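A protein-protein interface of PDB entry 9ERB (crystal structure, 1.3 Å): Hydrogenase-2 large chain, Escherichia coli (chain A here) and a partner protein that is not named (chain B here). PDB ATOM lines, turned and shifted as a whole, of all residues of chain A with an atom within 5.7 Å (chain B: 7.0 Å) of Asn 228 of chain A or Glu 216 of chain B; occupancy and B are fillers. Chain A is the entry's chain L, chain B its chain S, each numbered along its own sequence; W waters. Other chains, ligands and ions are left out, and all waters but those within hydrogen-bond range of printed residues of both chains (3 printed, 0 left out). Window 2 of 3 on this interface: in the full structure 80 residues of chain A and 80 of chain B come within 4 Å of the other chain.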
ATOM      1  N   PRO A 226      20.218  18.901 -18.268  1.00  0.00           N
ATOM      2  CA  PRO A 226      21.616  18.524 -18.545  1.00  0.00           C
ATOM      3  C   PRO A 226      22.552  19.468 -17.847  1.00  0.00           C
ATOM      4  O   PRO A 226      22.633  20.649 -18.192  1.00  0.00           O
ATOM      5  CB  PRO A 226      21.728  18.636 -20.074  1.00  0.00           C
ATOM      6  CG  PRO A 226      20.431  19.296 -20.576  1.00  0.00           C
ATOM      7  CD  PRO A 226      19.706  19.819 -19.323  1.00  0.00           C
ATOM      8  N   ILE A 227      23.206  18.997 -16.795  1.00  0.00           N
ATOM      9  CA  ILE A 227      24.120  19.844 -16.040  1.00  0.00           C
ATOM     10  C   ILE A 227      25.452  19.947 -16.768  1.00  0.00           C
ATOM     11  O   ILE A 227      26.147  18.941 -16.988  1.00  0.00           O
ATOM     12  CB  ILE A 227      24.340  19.308 -14.622  1.00  0.00           C
ATOM     13  CG1 ILE A 227      23.042  19.382 -13.811  1.00  0.00           C
ATOM     14  CG2 ILE A 227      25.461  20.076 -13.961  1.00  0.00           C
ATOM     15  CD1 ILE A 227      23.126  18.727 -12.426  1.00  0.00           C
ATOM     16  N   ASN A 228      25.819  21.168 -17.126  1.00  0.00           N
ATOM     17  CA  ASN A 228      27.111  21.418 -17.755  1.00  0.00           C
ATOM     18  C   ASN A 228      27.407  22.903 -17.579  1.00  0.00           C
ATOM     19  O   ASN A 228      26.885  23.725 -18.342  1.00  0.00           O
ATOM     20  CB  ASN A 228      27.058  21.050 -19.219  1.00  0.00           C
ATOM     21  CG  ASN A 228      28.397  21.220 -19.910  1.00  0.00           C
ATOM     22  OD1 ASN A 228      29.368  21.708 -19.296  1.00  0.00           O
ATOM     23  ND2 ASN A 228      28.459  20.835 -21.183  1.00  0.00           N
ATOM     24  N   LEU A 229      28.250  23.225 -16.602  1.00  0.00           N
ATOM     25  CA  LEU A 229      28.567  24.625 -16.322  1.00  0.00           C
ATOM     26  C   LEU A 229      29.064  25.350 -17.559  1.00  0.00           C
ATOM     27  O   LEU A 229      28.899  26.579 -17.670  1.00  0.00           O
ATOM     28  CB  LEU A 229      29.635  24.705 -15.238  1.00  0.00           C
ATOM     29  CG  LEU A 229      29.235  24.242 -13.842  1.00  0.00           C
ATOM     30  CD1 LEU A 229      30.373  24.478 -12.869  1.00  0.00           C
ATOM     31  CD2 LEU A 229      28.014  24.959 -13.336  1.00  0.00           C
ATOM     32  N   ASP A 230      29.670  24.632 -18.499  1.00  0.00           N
ATOM     33  CA  ASP A 230      30.333  25.240 -19.646  1.00  0.00           C
ATOM     34  C   ASP A 230      29.574  25.036 -20.943  1.00  0.00           C
ATOM     35  O   ASP A 230      30.088  25.374 -22.020  1.00  0.00           O
ATOM     36  CB  ASP A 230      31.755  24.694 -19.744  1.00  0.00           C
ATOM     37  CG  ASP A 230      32.580  25.106 -18.568  1.00  0.00           C
ATOM     38  OD1 ASP A 230      32.797  26.320 -18.354  1.00  0.00           O
ATOM     39  OD2 ASP A 230      32.941  24.195 -17.767  1.00  0.00           O
ATOM     40  N   GLY A 231      28.342  24.539 -20.886  1.00  0.00           N
ATOM     41  CA  GLY A 231      27.592  24.233 -22.089  1.00  0.00           C
ATOM     42  C   GLY A 231      26.641  25.346 -22.487  1.00  0.00           C
ATOM     43  O   GLY A 231      25.997  25.949 -21.649  1.00  0.00           O
ATOM     44  N   LEU A 232      26.520  25.558 -23.777  1.00  0.00           N
ATOM     45  CA  LEU A 232      25.528  26.467 -24.345  1.00  0.00           C
ATOM     46  C   LEU A 232      24.201  25.708 -24.457  1.00  0.00           C
ATOM     47  O   LEU A 232      24.168  24.541 -24.852  1.00  0.00           O
ATOM     48  CB  LEU A 232      26.053  26.945 -25.698  1.00  0.00           C
ATOM     49  CG  LEU A 232      25.252  28.019 -26.451  1.00  0.00           C
ATOM     50  CD1 LEU A 232      26.211  28.860 -27.286  1.00  0.00           C
ATOM     51  CD2 LEU A 232      24.209  27.373 -27.317  1.00  0.00           C
ATOM     52  N   VAL A 234      22.136  24.582 -22.091  1.00  0.00           N
ATOM     53  CA  VAL A 234      21.876  23.593 -21.056  1.00  0.00           C
ATOM     54  C   VAL A 234      21.942  24.246 -19.679  1.00  0.00           C
ATOM     55  O   VAL A 234      21.998  25.474 -19.564  1.00  0.00           O
ATOM     56  CB  VAL A 234      22.828  22.386 -21.193  1.00  0.00           C
ATOM     57  CG1 VAL A 234      22.680  21.765 -22.549  1.00  0.00           C
ATOM     58  CG2 VAL A 234      24.282  22.763 -20.942  1.00  0.00           C
ATOM     59  N   LEU A 235      21.899  23.448 -18.619  1.00  0.00           N
ATOM     60  CA  LEU A 235      21.877  23.986 -17.260  1.00  0.00           C
ATOM     61  C   LEU A 235      23.303  24.331 -16.844  1.00  0.00           C
ATOM     62  O   LEU A 235      24.070  23.501 -16.357  1.00  0.00           O
ATOM     63  CB  LEU A 235      21.197  23.023 -16.307  1.00  0.00           C
ATOM     64  CG  LEU A 235      21.020  23.461 -14.862  1.00  0.00           C
ATOM     65  CD1 LEU A 235      20.182  24.760 -14.797  1.00  0.00           C
ATOM     66  CD2 LEU A 235      20.361  22.414 -14.032  1.00  0.00           C
ATOM     67  N   ASN A 236      23.681  25.585 -17.112  1.00  0.00           N
ATOM     68  CA  ASN A 236      25.026  26.110 -16.875  1.00  0.00           C
ATOM     69  C   ASN A 236      25.011  27.080 -15.689  1.00  0.00           C
ATOM     70  O   ASN A 236      23.999  27.228 -14.999  1.00  0.00           O
ATOM     71  CB  ASN A 236      25.601  26.725 -18.151  1.00  0.00           C
ATOM     72  CG  ASN A 236      24.725  27.839 -18.689  1.00  0.00           C
ATOM     73  OD1 ASN A 236      24.072  28.554 -17.917  1.00  0.00           O
ATOM     74  ND2 ASN A 236      24.728  28.020 -19.997  1.00  0.00           N
ATOM     75  N   LEU A 237      26.142  27.726 -15.405  1.00  0.00           N
ATOM     76  CA  LEU A 237      26.180  28.602 -14.235  1.00  0.00           C
ATOM     77  C   LEU A 237      25.264  29.814 -14.406  1.00  0.00           C
ATOM     78  O   LEU A 237      24.624  30.257 -13.441  1.00  0.00           O
ATOM     79  CB  LEU A 237      27.620  28.993 -13.909  1.00  0.00           C
ATOM     80  CG  LEU A 237      27.799  29.736 -12.587  1.00  0.00           C
ATOM     81  CD1 LEU A 237      27.258  28.924 -11.422  1.00  0.00           C
ATOM     82  CD2 LEU A 237      29.270  30.097 -12.360  1.00  0.00           C
ATOM     83  N   HIS A 455      28.224  15.727 -12.500  1.00  0.00           N
ATOM     84  CA  HIS A 455      27.208  16.284 -13.384  1.00  0.00           C
ATOM     85  C   HIS A 455      26.123  15.259 -13.692  1.00  0.00           C
ATOM     86  O   HIS A 455      25.312  15.480 -14.589  1.00  0.00           O
ATOM     87  CB  HIS A 455      27.840  16.829 -14.669  1.00  0.00           C
ATOM     88  CG  HIS A 455      28.545  15.781 -15.474  1.00  0.00           C
ATOM     89  ND1 HIS A 455      29.917  15.768 -15.627  1.00  0.00           N
ATOM     90  CD2 HIS A 455      28.080  14.714 -16.160  1.00  0.00           C
ATOM     91  CE1 HIS A 455      30.262  14.734 -16.372  1.00  0.00           C
ATOM     92  NE2 HIS A 455      29.171  14.061 -16.689  1.00  0.00           N
ATOM     93  N   ARG B 196      16.817  23.753 -32.176  1.00  0.00           N
ATOM     94  CA  ARG B 196      17.663  22.572 -32.287  1.00  0.00           C
ATOM     95  C   ARG B 196      17.574  21.939 -33.661  1.00  0.00           C
ATOM     96  O   ARG B 196      18.230  20.914 -33.884  1.00  0.00           O
ATOM     97  CB  ARG B 196      17.353  21.564 -31.192  1.00  0.00           C
ATOM     98  CG  ARG B 196      17.527  22.239 -29.825  1.00  0.00           C
ATOM     99  CD  ARG B 196      17.506  21.289 -28.672  1.00  0.00           C
ATOM    100  NE  ARG B 196      17.754  22.008 -27.436  1.00  0.00           N
ATOM    101  CZ  ARG B 196      18.167  21.455 -26.316  1.00  0.00           C
ATOM    102  NH1 ARG B 196      18.354  20.155 -26.235  1.00  0.00           N
ATOM    103  NH2 ARG B 196      18.401  22.222 -25.266  1.00  0.00           N
ATOM    104  N   HIS B 199      20.873  20.760 -35.231  1.00  0.00           N
ATOM    105  CA  HIS B 199      21.357  19.483 -34.714  1.00  0.00           C
ATOM    106  C   HIS B 199      20.631  18.312 -35.363  1.00  0.00           C
ATOM    107  O   HIS B 199      21.270  17.328 -35.784  1.00  0.00           O
ATOM    108  CB  HIS B 199      21.230  19.457 -33.196  1.00  0.00           C
ATOM    109  CG  HIS B 199      21.909  20.614 -32.549  1.00  0.00           C
ATOM    110  ND1 HIS B 199      23.237  20.921 -32.777  1.00  0.00           N
ATOM    111  CD2 HIS B 199      21.428  21.592 -31.744  1.00  0.00           C
ATOM    112  CE1 HIS B 199      23.556  22.009 -32.101  1.00  0.00           C
ATOM    113  NE2 HIS B 199      22.469  22.432 -31.462  1.00  0.00           N
ATOM    114  N   ASP B 211      23.643  12.183 -21.361  1.00  0.00           N
ATOM    115  CA  ASP B 211      24.729  11.796 -22.266  1.00  0.00           C
ATOM    116  C   ASP B 211      25.399  13.036 -22.836  1.00  0.00           C
ATOM    117  O   ASP B 211      25.005  14.176 -22.548  1.00  0.00           O
ATOM    118  CB  ASP B 211      24.267  10.751 -23.275  1.00  0.00           C
ATOM    119  CG  ASP B 211      23.533  11.303 -24.496  1.00  0.00           C
ATOM    120  OD1 ASP B 211      23.374  12.535 -24.687  1.00  0.00           O
ATOM    121  OD2 ASP B 211      23.147  10.448 -25.329  1.00  0.00           O
ATOM    122  N   GLU B 212      26.486  12.816 -23.585  1.00  0.00           N
ATOM    123  CA  GLU B 212      27.290  13.957 -24.010  1.00  0.00           C
ATOM    124  C   GLU B 212      26.502  14.901 -24.899  1.00  0.00           C
ATOM    125  O   GLU B 212      26.570  16.122 -24.733  1.00  0.00           O
ATOM    126  CB  GLU B 212      28.533  13.501 -24.777  1.00  0.00           C
ATOM    127  CG  GLU B 212      29.726  13.164 -23.946  1.00  0.00           C
ATOM    128  CD  GLU B 212      30.988  12.986 -24.813  1.00  0.00           C
ATOM    129  OE1 GLU B 212      30.896  13.108 -26.054  1.00  0.00           O
ATOM    130  OE2 GLU B 212      32.061  12.730 -24.239  1.00  0.00           O
ATOM    131  N   GLY B 213      25.789  14.356 -25.876  1.00  0.00           N
ATOM    132  CA  GLY B 213      25.008  15.198 -26.776  1.00  0.00           C
ATOM    133  C   GLY B 213      23.906  15.942 -26.051  1.00  0.00           C
ATOM    134  O   GLY B 213      23.658  17.126 -26.313  1.00  0.00           O
ATOM    135  N   HIS B 214      23.244  15.270 -25.118  1.00  0.00           N
ATOM    136  CA  HIS B 214      22.226  15.926 -24.299  1.00  0.00           C
ATOM    137  C   HIS B 214      22.818  17.115 -23.559  1.00  0.00           C
ATOM    138  O   HIS B 214      22.202  18.195 -23.495  1.00  0.00           O
ATOM    139  CB  HIS B 214      21.667  14.908 -23.321  1.00  0.00           C
ATOM    140  CG  HIS B 214      20.495  15.396 -22.538  1.00  0.00           C
ATOM    141  ND1 HIS B 214      20.518  15.426 -21.164  1.00  0.00           N
ATOM    142  CD2 HIS B 214      19.289  15.897 -22.915  1.00  0.00           C
ATOM    143  CE1 HIS B 214      19.363  15.900 -20.721  1.00  0.00           C
ATOM    144  NE2 HIS B 214      18.596  16.173 -21.758  1.00  0.00           N
ATOM    145  N   ARG B 215      24.020  16.946 -23.013  1.00  0.00           N
ATOM    146  CA  ARG B 215      24.700  17.971 -22.246  1.00  0.00           C
ATOM    147  C   ARG B 215      25.334  19.039 -23.135  1.00  0.00           C
ATOM    148  O   ARG B 215      25.914  19.991 -22.613  1.00  0.00           O
ATOM    149  CB  ARG B 215      25.713  17.333 -21.303  1.00  0.00           C
ATOM    150  CG  ARG B 215      24.996  16.606 -20.177  1.00  0.00           C
ATOM    151  CD  ARG B 215      25.953  15.819 -19.296  1.00  0.00           C
ATOM    152  NE  ARG B 215      26.762  16.770 -18.558  1.00  0.00           N
ATOM    153  CZ  ARG B 215      28.074  16.926 -18.703  1.00  0.00           C
ATOM    154  NH1 ARG B 215      28.789  16.093 -19.467  1.00  0.00           N
ATOM    155  NH2 ARG B 215      28.676  17.947 -18.086  1.00  0.00           N
ATOM    156  N   GLU B 216      25.190  18.913 -24.450  1.00  0.00           N
ATOM    157  CA  GLU B 216      25.542  19.972 -25.378  1.00  0.00           C
ATOM    158  C   GLU B 216      24.324  20.619 -26.013  1.00  0.00           C
ATOM    159  O   GLU B 216      24.487  21.471 -26.895  1.00  0.00           O
ATOM    160  CB  GLU B 216      26.495  19.432 -26.447  1.00  0.00           C
ATOM    161  CG  GLU B 216      27.876  18.997 -25.880  1.00  0.00           C
ATOM    162  CD  GLU B 216      28.695  20.057 -25.110  1.00  0.00           C
ATOM    163  OE1 GLU B 216      28.528  21.293 -25.286  1.00  0.00           O
ATOM    164  OE2 GLU B 216      29.551  19.638 -24.288  1.00  0.00           O
ATOM    165  N   GLY B 217      23.115  20.236 -25.617  1.00  0.00           N
ATOM    166  CA  GLY B 217      21.946  20.895 -26.165  1.00  0.00           C
ATOM    167  C   GLY B 217      21.544  20.410 -27.532  1.00  0.00           C
ATOM    168  O   GLY B 217      20.898  21.150 -28.297  1.00  0.00           O
ATOM    169  N   TRP B 218      21.842  19.158 -27.848  1.00  0.00           N
ATOM    170  CA  TRP B 218      21.524  18.608 -29.160  1.00  0.00           C
ATOM    171  C   TRP B 218      20.035  18.269 -29.298  1.00  0.00           C
ATOM    172  O   TRP B 218      19.243  18.395 -28.353  1.00  0.00           O
ATOM    173  CB  TRP B 218      22.400  17.385 -29.427  1.00  0.00           C
ATOM    174  CG  TRP B 218      23.845  17.673 -29.709  1.00  0.00           C
ATOM    175  CD1 TRP B 218      24.450  18.869 -29.719  1.00  0.00           C
ATOM    176  CD2 TRP B 218      24.867  16.692 -30.018  1.00  0.00           C
ATOM    177  NE1 TRP B 218      25.798  18.721 -30.018  1.00  0.00           N
ATOM    178  CE2 TRP B 218      26.065  17.389 -30.183  1.00  0.00           C
ATOM    179  CE3 TRP B 218      24.864  15.306 -30.176  1.00  0.00           C
ATOM    180  CZ2 TRP B 218      27.269  16.752 -30.546  1.00  0.00           C
ATOM    181  CZ3 TRP B 218      26.058  14.665 -30.507  1.00  0.00           C
ATOM    182  CH2 TRP B 218      27.236  15.393 -30.686  1.00  0.00           C
HETATM  183  O   HOH W   1      30.565  23.120 -24.399  1.00  0.00           O
HETATM  184  O   HOH W   2      26.736  23.352 -25.793  1.00  0.00           O
HETATM  185  O   HOH W   3      30.999  21.072 -22.810  1.00  0.00           O
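Of the 10 printed residues of chain B, 4 touch a printed residue of chain A.
Printed residues of chain B that touch a printed residue of chain A: His 214, Arg 215, Glu 216 and Gly 217.
Hydrophobic or aromatic side chains of chain B that line the printed part of chain A: His 214.
Printed residues of chain A that touch a printed residue of chain B: Pro 226, Ile 227, Asn 228, Leu 232, Val 234 and His 455.
Among the printed residues, 10 pairs touch across the chains.
Among the printed residues, no Asp or Glu carboxylate lies within 4 Å of a Lys or Arg side-chain nitrogen of the other chain.
Of the printed residues of chain B, Ile 227 of chain A touches Arg 215 (2.7 Å).
Asn 228 of chain A touches just these residues of chain B: Arg 215 and Glu 216.
Of the printed residues of chain B, His 455 of chain A touches Arg 215 (3.4 Å).
Gly 213 of chain B touches none of the printed residues of chain A.
Printed residues of chain A within 4 Å of Gly 217 of chain B: Val 234.
The nearest printed residue of chain A that does not touch Glu 216 of chain B is Val 234 of chain A (4.002 Å).
The nearest printed residue of chain B that does not touch Pro 226 of chain A is Glu 216 of chain B (5.6 Å).
Water W3 lies within hydrogen-bond range of the side-chain carboxylate (OE2) of Glu 216 of chain B (2.5 Å) and the side-chain amide nitrogen (ND2) of Asn 228 of chain A (3.0 Å).
Water W2 bridges OE1 of Glu 216 of chain B (2.8 Å) and O of Leu 232 of chain A (3.0 Å).
Water W1 lies within hydrogen-bond range of the side-chain carboxylate of Glu 216 of chain B (2.9 Å) and the backbone carbonyl oxygen of Asp 230 of chain A (3.3 Å).
The guanidinium group (NE) of Arg 196 of chain B sits at hydrogen-bond distance from the backbone carbonyl oxygen (O) of Gly 217 of chain B (3.4 Å).
The backbone NH (N) of His 214 of chain B lies within hydrogen-bond range of the side-chain carboxylate (OD1) of Asp 211 of chain B, 2.8 Å away.
The backbone NH (N) of Leu 235 of chain A is in hydrogen-bond range of the backbone carbonyl oxygen (O) of Pro 226 of chain A, at 2.9 Å.
The side-chain amide oxygen of Asn 228 of chain A sits close to the backbone NH of Asp 230 of chain A (3.0 Å).
OD1 of Asn 228 of chain A sits at hydrogen-bond distance from N of Gly 231 of chain A (3.4 Å).
N of Asn 228 of chain A lies within hydrogen-bond range of O of Leu 235 of chain A, 3.0 Å away.
Among the printed residues, merely in contact across the chains: Pro 226 of chain A with His 214 of chain B (3.5 Å), Pro 226 of chain A with Arg 215 of chain B (3.7 Å), Asn 228 of chain A with Glu 216 of chain B (3.5 Å), Leu 232 of chain A with Glu 216 of chain B (3.7 Å), Val 234 of chain A with His 214 of chain B (3.7 Å), Val 234 of chain A with Arg 215 of chain B (3.6 Å) and Val 234 of chain A with Gly 217 of chain B (3.5 Å).
The guanidinium group (NE) of Arg 215 of chain B sits at hydrogen-bond distance from the backbone carbonyl oxygen (O) of Ile 227 of chain A.
The backbone carbonyl oxygen of Arg 215 of chain B lies within hydrogen-bond range of the side-chain amide nitrogen of Asn 228 of chain A, at 3.0 Å.
The guanidinium group (NH1) of Arg 215 of chain B lies within hydrogen-bond range of a ring nitrogen (NE2) of His 455 of chain A.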
